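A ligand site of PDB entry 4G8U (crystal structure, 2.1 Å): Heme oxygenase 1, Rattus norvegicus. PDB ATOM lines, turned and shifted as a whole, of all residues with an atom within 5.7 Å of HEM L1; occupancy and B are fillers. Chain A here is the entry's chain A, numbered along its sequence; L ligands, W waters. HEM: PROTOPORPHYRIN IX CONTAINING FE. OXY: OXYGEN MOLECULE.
NE2 of His 25 is bound to FE of HEM L1. The side-chain amino group (NZ) of Lys 179 is in salt-bridge range of an oxygen (O1A) of HEM L1 (2.5 Å). O2D of HEM L1 lies within hydrogen-bond range of OH of Tyr 134. NH2 of Arg 183 is in salt-bridge range of O1D of HEM L1 (2.9 Å). The backbone NH of Gly 143 is in hydrogen-bond range of an oxygen (O2) of OXY L2, at 3.0 Å. The backbone carbonyl oxygen of Gly 139 sits close to an oxygen (O2) of OXY L2, at 2.7 Å. An oxygen (O2) of OXY L2 lies within hydrogen-bond range of the backbone NH of Gly 144, 3.5 Å away.
An iron atom (FE) of HEM L1 is bound by an oxygen (O1) of OXY L2 (1.9 Å).
ND1 of His 25 lies within hydrogen-bond range of OE1 of Glu 29. The side-chain amino group (NZ) of Lys 179 is in hydrogen-bond range of the side-chain hydroxyl (OG) of Ser 142 (2.9 Å). The side-chain hydroxyl of Tyr 134 lies within hydrogen-bond range of the side-chain hydroxyl of Thr 21 (3.4 Å). OE1 of Gln 38 lies close to O of Glu 29, at 3.2 Å. The side-chain amide oxygen (OD1) of Asn 210 is in hydrogen-bond range of the guanidinium group (NH1) of Arg 136, 2.9 Å away. ND2 of Asn 210 sits at hydrogen-bond distance from O of Ala 206, at 2.8 Å. O of Gly 139 is in hydrogen-bond range of N of Gly 144 (3.0 Å). The backbone carbonyl oxygen (O) of Leu 138 lies within hydrogen-bond range of the side-chain hydroxyl (OG) of Ser 142.
Merely in contact with HEM L1: Lys 18, Ala 28, Glu 29, Gln 38, Thr 135, Arg 136, Leu 138, Gly 139, Ser 142, Gly 143, Leu 147, Phe 207, Asn 210 and Phe 214. Hydrophobic or aromatic side chains that line HEM L1: His 25, Ala 28, Tyr 134, Leu 138, Leu 147, Phe 207 and Phe 214. Of the 25 residues printed, 18 come within 4 Å of HEM L1. Along chain A the residues within 4 Å of HEM L1 span positions 18 to 214.
Water W3 lies within hydrogen-bond range of O2D of HEM L1 (2.5 Å), O of Ser 14 (2.7 Å) and NE of Arg 183 (3.3 Å).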
ATOM      1  N   SER A  14     -13.642 -17.979  21.536  1.00  0.00           N
ATOM      2  CA  SER A  14     -14.562 -17.127  20.809  1.00  0.00           C
ATOM      3  C   SER A  14     -14.225 -17.051  19.303  1.00  0.00           C
ATOM      4  O   SER A  14     -15.105 -17.064  18.465  1.00  0.00           O
ATOM      5  CB  SER A  14     -14.577 -15.707  21.371  1.00  0.00           C
ATOM      6  OG  SER A  14     -13.311 -15.110  21.117  1.00  0.00           O
ATOM      7  N   LEU A  17     -14.866 -20.520  17.553  1.00  0.00           N
ATOM      8  CA  LEU A  17     -16.284 -20.722  17.314  1.00  0.00           C
ATOM      9  C   LEU A  17     -16.748 -19.898  16.124  1.00  0.00           C
ATOM     10  O   LEU A  17     -17.495 -20.408  15.257  1.00  0.00           O
ATOM     11  CB  LEU A  17     -17.090 -20.381  18.562  1.00  0.00           C
ATOM     12  CG  LEU A  17     -17.215 -21.377  19.673  1.00  0.00           C
ATOM     13  CD1 LEU A  17     -17.795 -20.717  20.953  1.00  0.00           C
ATOM     14  CD2 LEU A  17     -18.208 -22.380  19.149  1.00  0.00           C
ATOM     15  N   LYS A  18     -16.334 -18.635  16.056  1.00  0.00           N
ATOM     16  CA  LYS A  18     -16.698 -17.825  14.869  1.00  0.00           C
ATOM     17  C   LYS A  18     -16.227 -18.455  13.580  1.00  0.00           C
ATOM     18  O   LYS A  18     -16.991 -18.537  12.606  1.00  0.00           O
ATOM     19  CB  LYS A  18     -16.197 -16.375  14.927  1.00  0.00           C
ATOM     20  CG  LYS A  18     -17.038 -15.448  14.019  1.00  0.00           C
ATOM     21  CD  LYS A  18     -16.508 -14.033  14.071  1.00  0.00           C
ATOM     22  CE  LYS A  18     -17.282 -13.068  13.189  1.00  0.00           C
ATOM     23  NZ  LYS A  18     -16.596 -11.745  13.267  1.00  0.00           N
ATOM     24  N   THR A  21     -18.117 -21.789  12.688  1.00  0.00           N
ATOM     25  CA  THR A  21     -19.520 -21.657  12.337  1.00  0.00           C
ATOM     26  C   THR A  21     -19.874 -20.641  11.254  1.00  0.00           C
ATOM     27  O   THR A  21     -21.057 -20.525  10.871  1.00  0.00           O
ATOM     28  CB  THR A  21     -20.429 -21.419  13.604  1.00  0.00           C
ATOM     29  OG1 THR A  21     -20.194 -20.104  14.141  1.00  0.00           O
ATOM     30  CG2 THR A  21     -20.165 -22.529  14.677  1.00  0.00           C
ATOM     31  N   HIS A  25     -23.297 -20.566   9.166  1.00  0.00           N
ATOM     32  CA  HIS A  25     -24.129 -19.374   9.444  1.00  0.00           C
ATOM     33  C   HIS A  25     -24.687 -18.872   8.138  1.00  0.00           C
ATOM     34  O   HIS A  25     -25.881 -18.556   8.007  1.00  0.00           O
ATOM     35  CB  HIS A  25     -23.325 -18.281  10.150  1.00  0.00           C
ATOM     36  CG  HIS A  25     -24.145 -17.090  10.534  1.00  0.00           C
ATOM     37  ND1 HIS A  25     -24.580 -16.186   9.606  1.00  0.00           N
ATOM     38  CD2 HIS A  25     -24.725 -16.736  11.752  1.00  0.00           C
ATOM     39  CE1 HIS A  25     -25.372 -15.290  10.229  1.00  0.00           C
ATOM     40  NE2 HIS A  25     -25.398 -15.572  11.548  1.00  0.00           N
ATOM     41  N   ALA A  28     -27.480 -21.061   7.192  1.00  0.00           N
ATOM     42  CA  ALA A  28     -28.632 -20.802   8.061  1.00  0.00           C
ATOM     43  C   ALA A  28     -29.322 -19.475   7.670  1.00  0.00           C
ATOM     44  O   ALA A  28     -30.543 -19.449   7.496  1.00  0.00           O
ATOM     45  CB  ALA A  28     -28.207 -20.789   9.511  1.00  0.00           C
ATOM     46  N   GLU A  29     -28.573 -18.396   7.496  1.00  0.00           N
ATOM     47  CA  GLU A  29     -29.221 -17.139   7.147  1.00  0.00           C
ATOM     48  C   GLU A  29     -29.889 -17.185   5.796  1.00  0.00           C
ATOM     49  O   GLU A  29     -30.733 -16.359   5.525  1.00  0.00           O
ATOM     50  CB  GLU A  29     -28.317 -15.913   7.371  1.00  0.00           C
ATOM     51  CG  GLU A  29     -27.251 -15.723   6.338  1.00  0.00           C
ATOM     52  CD  GLU A  29     -26.181 -14.788   6.821  1.00  0.00           C
ATOM     53  OE1 GLU A  29     -24.985 -15.213   6.922  1.00  0.00           O
ATOM     54  OE2 GLU A  29     -26.566 -13.613   7.033  1.00  0.00           O
ATOM     55  N   MET A  34     -35.851 -18.264   6.312  1.00  0.00           N
ATOM     56  CA  MET A  34     -35.224 -17.009   6.724  1.00  0.00           C
ATOM     57  C   MET A  34     -35.187 -16.032   5.600  1.00  0.00           C
ATOM     58  O   MET A  34     -35.430 -14.861   5.835  1.00  0.00           O
ATOM     59  CB  MET A  34     -33.815 -17.183   7.274  1.00  0.00           C
ATOM     60  CG  MET A  34     -33.763 -17.811   8.624  1.00  0.00           C
ATOM     61  SD  MET A  34     -34.667 -16.706   9.744  1.00  0.00           S
ATOM     62  CE  MET A  34     -34.961 -17.673  11.228  1.00  0.00           C
ATOM     63  N   GLN A  38     -36.774 -12.425   5.869  1.00  0.00           N
ATOM     64  CA  GLN A  38     -35.959 -11.217   5.609  1.00  0.00           C
ATOM     65  C   GLN A  38     -36.589 -10.363   4.533  1.00  0.00           C
ATOM     66  O   GLN A  38     -36.486  -9.173   4.598  1.00  0.00           O
ATOM     67  CB  GLN A  38     -34.533 -11.592   5.164  1.00  0.00           C
ATOM     68  CG  GLN A  38     -33.401 -11.475   6.169  1.00  0.00           C
ATOM     69  CD  GLN A  38     -32.229 -12.405   5.821  1.00  0.00           C
ATOM     70  OE1 GLN A  38     -32.424 -13.599   5.664  1.00  0.00           O
ATOM     71  NE2 GLN A  38     -31.007 -11.855   5.705  1.00  0.00           N
ATOM     72  N   TYR A 134     -24.132 -20.148  23.088  1.00  0.00           N
ATOM     73  CA  TYR A 134     -23.525 -19.321  22.063  1.00  0.00           C
ATOM     74  C   TYR A 134     -24.357 -19.188  20.795  1.00  0.00           C
ATOM     75  O   TYR A 134     -24.700 -18.093  20.314  1.00  0.00           O
ATOM     76  CB  TYR A 134     -22.170 -19.928  21.729  1.00  0.00           C
ATOM     77  CG  TYR A 134     -21.584 -19.438  20.466  1.00  0.00           C
ATOM     78  CD1 TYR A 134     -20.959 -18.194  20.403  1.00  0.00           C
ATOM     79  CD2 TYR A 134     -21.608 -20.222  19.323  1.00  0.00           C
ATOM     80  CE1 TYR A 134     -20.344 -17.746  19.239  1.00  0.00           C
ATOM     81  CE2 TYR A 134     -21.044 -19.759  18.151  1.00  0.00           C
ATOM     82  CZ  TYR A 134     -20.409 -18.518  18.098  1.00  0.00           C
ATOM     83  OH  TYR A 134     -19.820 -18.065  16.890  1.00  0.00           O
ATOM     84  N   THR A 135     -24.694 -20.352  20.265  1.00  0.00           N
ATOM     85  CA  THR A 135     -25.355 -20.385  18.972  1.00  0.00           C
ATOM     86  C   THR A 135     -26.682 -19.637  18.992  1.00  0.00           C
ATOM     87  O   THR A 135     -27.064 -18.913  18.053  1.00  0.00           O
ATOM     88  CB  THR A 135     -25.581 -21.844  18.526  1.00  0.00           C
ATOM     89  OG1 THR A 135     -24.297 -22.481  18.320  1.00  0.00           O
ATOM     90  CG2 THR A 135     -26.515 -21.895  17.255  1.00  0.00           C
ATOM     91  N   ARG A 136     -27.448 -19.818  20.062  1.00  0.00           N
ATOM     92  CA  ARG A 136     -28.750 -19.137  20.090  1.00  0.00           C
ATOM     93  C   ARG A 136     -28.616 -17.684  20.600  1.00  0.00           C
ATOM     94  O   ARG A 136     -29.095 -16.772  19.950  1.00  0.00           O
ATOM     95  CB  ARG A 136     -29.726 -19.881  20.979  1.00  0.00           C
ATOM     96  CG  ARG A 136     -30.316 -21.124  20.349  1.00  0.00           C
ATOM     97  CD  ARG A 136     -31.023 -20.876  18.995  1.00  0.00           C
ATOM     98  NE  ARG A 136     -31.775 -19.628  18.977  1.00  0.00           N
ATOM     99  CZ  ARG A 136     -32.396 -19.111  17.901  1.00  0.00           C
ATOM    100  NH1 ARG A 136     -32.363 -19.730  16.748  1.00  0.00           N
ATOM    101  NH2 ARG A 136     -33.000 -17.917  17.927  1.00  0.00           N
ATOM    102  N   LEU A 138     -26.170 -15.417  21.042  1.00  0.00           N
ATOM    103  CA  LEU A 138     -25.457 -14.417  20.241  1.00  0.00           C
ATOM    104  C   LEU A 138     -26.147 -14.093  18.931  1.00  0.00           C
ATOM    105  O   LEU A 138     -26.062 -12.962  18.456  1.00  0.00           O
ATOM    106  CB  LEU A 138     -23.989 -14.785  20.033  1.00  0.00           C
ATOM    107  CG  LEU A 138     -23.010 -14.840  21.245  1.00  0.00           C
ATOM    108  CD1 LEU A 138     -21.600 -14.397  20.845  1.00  0.00           C
ATOM    109  CD2 LEU A 138     -23.462 -14.061  22.476  1.00  0.00           C
ATOM    110  N   GLY A 139     -26.793 -15.070  18.317  1.00  0.00           N
ATOM    111  CA  GLY A 139     -27.613 -14.777  17.160  1.00  0.00           C
ATOM    112  C   GLY A 139     -28.783 -13.865  17.521  1.00  0.00           C
ATOM    113  O   GLY A 139     -29.154 -12.969  16.727  1.00  0.00           O
ATOM    114  N   SER A 142     -27.912 -10.464  17.362  1.00  0.00           N
ATOM    115  CA  SER A 142     -27.355 -10.022  16.113  1.00  0.00           C
ATOM    116  C   SER A 142     -28.456  -9.983  15.051  1.00  0.00           C
ATOM    117  O   SER A 142     -29.298  -9.073  15.027  1.00  0.00           O
ATOM    118  CB  SER A 142     -26.200 -10.938  15.765  1.00  0.00           C
ATOM    119  OG  SER A 142     -25.270 -11.049  16.809  1.00  0.00           O
ATOM    120  N   GLY A 143     -28.499 -11.017  14.214  1.00  0.00           N
ATOM    121  CA  GLY A 143     -29.592 -11.186  13.237  1.00  0.00           C
ATOM    122  C   GLY A 143     -31.004 -11.102  13.828  1.00  0.00           C
ATOM    123  O   GLY A 143     -31.923 -10.570  13.192  1.00  0.00           O
ATOM    124  N   GLY A 144     -31.166 -11.615  15.045  1.00  0.00           N
ATOM    125  CA  GLY A 144     -32.464 -11.522  15.739  1.00  0.00           C
ATOM    126  C   GLY A 144     -32.944 -10.075  15.816  1.00  0.00           C
ATOM    127  O   GLY A 144     -34.142  -9.805  15.666  1.00  0.00           O
ATOM    128  N   VAL A 146     -32.303  -7.710  13.633  1.00  0.00           N
ATOM    129  CA  VAL A 146     -32.735  -7.342  12.292  1.00  0.00           C
ATOM    130  C   VAL A 146     -34.080  -7.986  12.034  1.00  0.00           C
ATOM    131  O   VAL A 146     -34.987  -7.351  11.552  1.00  0.00           O
ATOM    132  CB  VAL A 146     -31.730  -7.810  11.267  1.00  0.00           C
ATOM    133  CG1 VAL A 146     -32.334  -7.591   9.869  1.00  0.00           C
ATOM    134  CG2 VAL A 146     -30.379  -7.124  11.531  1.00  0.00           C
ATOM    135  N   LEU A 147     -34.238  -9.246  12.415  1.00  0.00           N
ATOM    136  CA  LEU A 147     -35.498  -9.894  12.206  1.00  0.00           C
ATOM    137  C   LEU A 147     -36.636  -9.234  13.011  1.00  0.00           C
ATOM    138  O   LEU A 147     -37.766  -9.131  12.576  1.00  0.00           O
ATOM    139  CB  LEU A 147     -35.429 -11.370  12.535  1.00  0.00           C
ATOM    140  CG  LEU A 147     -34.513 -12.302  11.716  1.00  0.00           C
ATOM    141  CD1 LEU A 147     -34.523 -13.714  12.333  1.00  0.00           C
ATOM    142  CD2 LEU A 147     -34.928 -12.288  10.224  1.00  0.00           C
ATOM    143  N   LYS A 179     -22.131  -8.574  23.649  1.00  0.00           N
ATOM    144  CA  LYS A 179     -21.542  -9.669  22.885  1.00  0.00           C
ATOM    145  C   LYS A 179     -20.050  -9.691  23.063  1.00  0.00           C
ATOM    146  O   LYS A 179     -19.451 -10.727  23.203  1.00  0.00           O
ATOM    147  CB  LYS A 179     -21.873  -9.561  21.379  1.00  0.00           C
ATOM    148  CG  LYS A 179     -23.275 -10.063  21.036  1.00  0.00           C
ATOM    149  CD  LYS A 179     -23.659  -9.951  19.562  1.00  0.00           C
ATOM    150  CE  LYS A 179     -23.754  -8.538  19.013  1.00  0.00           C
ATOM    151  NZ  LYS A 179     -23.736  -8.657  17.497  1.00  0.00           N
ATOM    152  N   ARG A 183     -18.091 -12.914  24.591  1.00  0.00           N
ATOM    153  CA  ARG A 183     -16.923 -13.553  23.921  1.00  0.00           C
ATOM    154  C   ARG A 183     -15.715 -13.637  24.860  1.00  0.00           C
ATOM    155  O   ARG A 183     -15.065 -14.659  24.955  1.00  0.00           O
ATOM    156  CB  ARG A 183     -16.547 -12.790  22.640  1.00  0.00           C
ATOM    157  CG  ARG A 183     -17.553 -12.937  21.490  1.00  0.00           C
ATOM    158  CD  ARG A 183     -17.082 -12.194  20.234  1.00  0.00           C
ATOM    159  NE  ARG A 183     -18.140 -12.110  19.253  1.00  0.00           N
ATOM    160  CZ  ARG A 183     -18.888 -11.023  19.001  1.00  0.00           C
ATOM    161  NH1 ARG A 183     -18.706  -9.905  19.682  1.00  0.00           N
ATOM    162  NH2 ARG A 183     -19.893 -11.087  18.128  1.00  0.00           N
ATOM    163  N   ALA A 206     -25.484 -27.440  16.572  1.00  0.00           N
ATOM    164  CA  ALA A 206     -26.536 -26.520  16.962  1.00  0.00           C
ATOM    165  C   ALA A 206     -27.101 -25.809  15.699  1.00  0.00           C
ATOM    166  O   ALA A 206     -28.308 -25.669  15.513  1.00  0.00           O
ATOM    167  CB  ALA A 206     -25.995 -25.470  17.960  1.00  0.00           C
ATOM    168  N   PHE A 207     -26.195 -25.310  14.888  1.00  0.00           N
ATOM    169  CA  PHE A 207     -26.599 -24.596  13.702  1.00  0.00           C
ATOM    170  C   PHE A 207     -27.392 -25.530  12.822  1.00  0.00           C
ATOM    171  O   PHE A 207     -28.425 -25.121  12.328  1.00  0.00           O
ATOM    172  CB  PHE A 207     -25.421 -24.031  12.961  1.00  0.00           C
ATOM    173  CG  PHE A 207     -25.100 -22.625  13.314  1.00  0.00           C
ATOM    174  CD1 PHE A 207     -24.181 -22.323  14.301  1.00  0.00           C
ATOM    175  CD2 PHE A 207     -25.646 -21.584  12.595  1.00  0.00           C
ATOM    176  CE1 PHE A 207     -23.847 -21.041  14.599  1.00  0.00           C
ATOM    177  CE2 PHE A 207     -25.335 -20.266  12.894  1.00  0.00           C
ATOM    178  CZ  PHE A 207     -24.433 -19.992  13.899  1.00  0.00           C
ATOM    179  N   ASN A 210     -30.953 -25.932  13.989  1.00  0.00           N
ATOM    180  CA  ASN A 210     -31.727 -24.769  13.652  1.00  0.00           C
ATOM    181  C   ASN A 210     -32.153 -24.818  12.174  1.00  0.00           C
ATOM    182  O   ASN A 210     -33.324 -24.535  11.825  1.00  0.00           O
ATOM    183  CB  ASN A 210     -30.901 -23.477  13.947  1.00  0.00           C
ATOM    184  CG  ASN A 210     -30.958 -23.086  15.406  1.00  0.00           C
ATOM    185  OD1 ASN A 210     -31.943 -22.496  15.852  1.00  0.00           O
ATOM    186  ND2 ASN A 210     -29.950 -23.519  16.192  1.00  0.00           N
ATOM    187  N   PHE A 214     -35.994 -24.955  10.568  1.00  0.00           N
ATOM    188  CA  PHE A 214     -36.531 -24.053   9.536  1.00  0.00           C
ATOM    189  C   PHE A 214     -36.970 -24.720   8.289  1.00  0.00           C
ATOM    190  O   PHE A 214     -37.995 -24.315   7.679  1.00  0.00           O
ATOM    191  CB  PHE A 214     -35.529 -22.976   9.155  1.00  0.00           C
ATOM    192  CG  PHE A 214     -35.094 -22.133  10.326  1.00  0.00           C
ATOM    193  CD1 PHE A 214     -35.995 -21.777  11.311  1.00  0.00           C
ATOM    194  CD2 PHE A 214     -33.794 -21.687  10.424  1.00  0.00           C
ATOM    195  CE1 PHE A 214     -35.611 -21.007  12.401  1.00  0.00           C
ATOM    196  CE2 PHE A 214     -33.410 -20.917  11.513  1.00  0.00           C
ATOM    197  CZ  PHE A 214     -34.310 -20.589  12.491  1.00  0.00           C
HETATM  198  CHA HEM L   1     -23.754 -13.339  14.268  1.00  0.00           C
HETATM  199  CHB HEM L   1     -27.019 -11.878  10.916  1.00  0.00           C
HETATM  200  CHC HEM L   1     -29.377 -16.029  11.463  1.00  0.00           C
HETATM  201  CHD HEM L   1     -26.303 -17.268  15.053  1.00  0.00           C
HETATM  202  C1A HEM L   1     -24.399 -12.545  13.250  1.00  0.00           C
HETATM  203  C2A HEM L   1     -23.895 -11.219  12.759  1.00  0.00           C
HETATM  204  C3A HEM L   1     -24.900 -10.801  11.769  1.00  0.00           C
HETATM  205  C4A HEM L   1     -25.889 -11.907  11.765  1.00  0.00           C
HETATM  206  CMA HEM L   1     -24.900  -9.489  10.938  1.00  0.00           C
HETATM  207  CAA HEM L   1     -22.601 -10.513  13.259  1.00  0.00           C
HETATM  208  CBA HEM L   1     -22.643  -9.985  14.731  1.00  0.00           C
HETATM  209  CGA HEM L   1     -21.343  -9.539  15.470  1.00  0.00           C
HETATM  210  O1A HEM L   1     -21.455  -9.106  16.677  1.00  0.00           O
HETATM  211  O2A HEM L   1     -20.205  -9.601  14.913  1.00  0.00           O
HETATM  212  C1B HEM L   1     -28.005 -12.924  10.778  1.00  0.00           C
HETATM  213  C2B HEM L   1     -29.133 -12.730   9.842  1.00  0.00           C
HETATM  214  C3B HEM L   1     -29.821 -13.980  10.081  1.00  0.00           C
HETATM  215  C4B HEM L   1     -29.013 -14.697  11.047  1.00  0.00           C
HETATM  216  CMB HEM L   1     -29.502 -11.559   8.963  1.00  0.00           C
HETATM  217  CAB HEM L   1     -31.031 -14.572   9.494  1.00  0.00           C
HETATM  218  CBB HEM L   1     -31.778 -13.936   8.637  1.00  0.00           C
HETATM  219  C1C HEM L   1     -28.695 -16.785  12.428  1.00  0.00           C
HETATM  220  C2C HEM L   1     -29.234 -18.104  12.864  1.00  0.00           C
HETATM  221  C3C HEM L   1     -28.299 -18.375  13.929  1.00  0.00           C
HETATM  222  C4C HEM L   1     -27.375 -17.259  14.125  1.00  0.00           C
HETATM  223  CMC HEM L   1     -30.353 -18.984  12.342  1.00  0.00           C
HETATM  224  CAC HEM L   1     -28.207 -19.565  14.777  1.00  0.00           C
HETATM  225  CBC HEM L   1     -29.088 -20.465  14.727  1.00  0.00           C
HETATM  226  C1D HEM L   1     -25.289 -16.279  15.160  1.00  0.00           C
HETATM  227  C2D HEM L   1     -24.208 -16.439  16.129  1.00  0.00           C
HETATM  228  C3D HEM L   1     -23.464 -15.225  15.868  1.00  0.00           C
HETATM  229  C4D HEM L   1     -24.239 -14.581  14.823  1.00  0.00           C
HETATM  230  CMD HEM L   1     -23.967 -17.547  17.115  1.00  0.00           C
HETATM  231  CAD HEM L   1     -22.197 -14.713  16.479  1.00  0.00           C
HETATM  232  CBD HEM L   1     -20.989 -15.191  15.686  1.00  0.00           C
HETATM  233  CGD HEM L   1     -19.760 -14.768  16.476  1.00  0.00           C
HETATM  234  O1D HEM L   1     -19.618 -13.575  16.712  1.00  0.00           O
HETATM  235  O2D HEM L   1     -18.954 -15.600  16.920  1.00  0.00           O
HETATM  236  NA  HEM L   1     -25.591 -13.003  12.633  1.00  0.00           N
HETATM  237  NB  HEM L   1     -27.949 -14.069  11.444  1.00  0.00           N
HETATM  238  NC  HEM L   1     -27.622 -16.282  13.187  1.00  0.00           N
HETATM  239  ND  HEM L   1     -25.281 -15.243  14.395  1.00  0.00           N
HETATM  240 FE   HEM L   1     -26.617 -14.680  12.925  1.00  0.00          FE
HETATM  241  O1  OXY L   2     -27.706 -13.771  14.175  1.00  0.00           O
HETATM  242  O2  OXY L   2     -28.813 -14.015  14.207  1.00  0.00           O
HETATM  243  O   HOH W   1     -30.564 -15.868  15.167  1.00  0.00           O
HETATM  244  O   HOH W   2     -22.413 -14.007  11.369  1.00  0.00           O
HETATM  245  O   HOH W   3     -17.029 -15.139  18.420  1.00  0.00           O
HETATM  246  O   HOH W   4     -29.564 -17.509  17.195  1.00  0.00           O
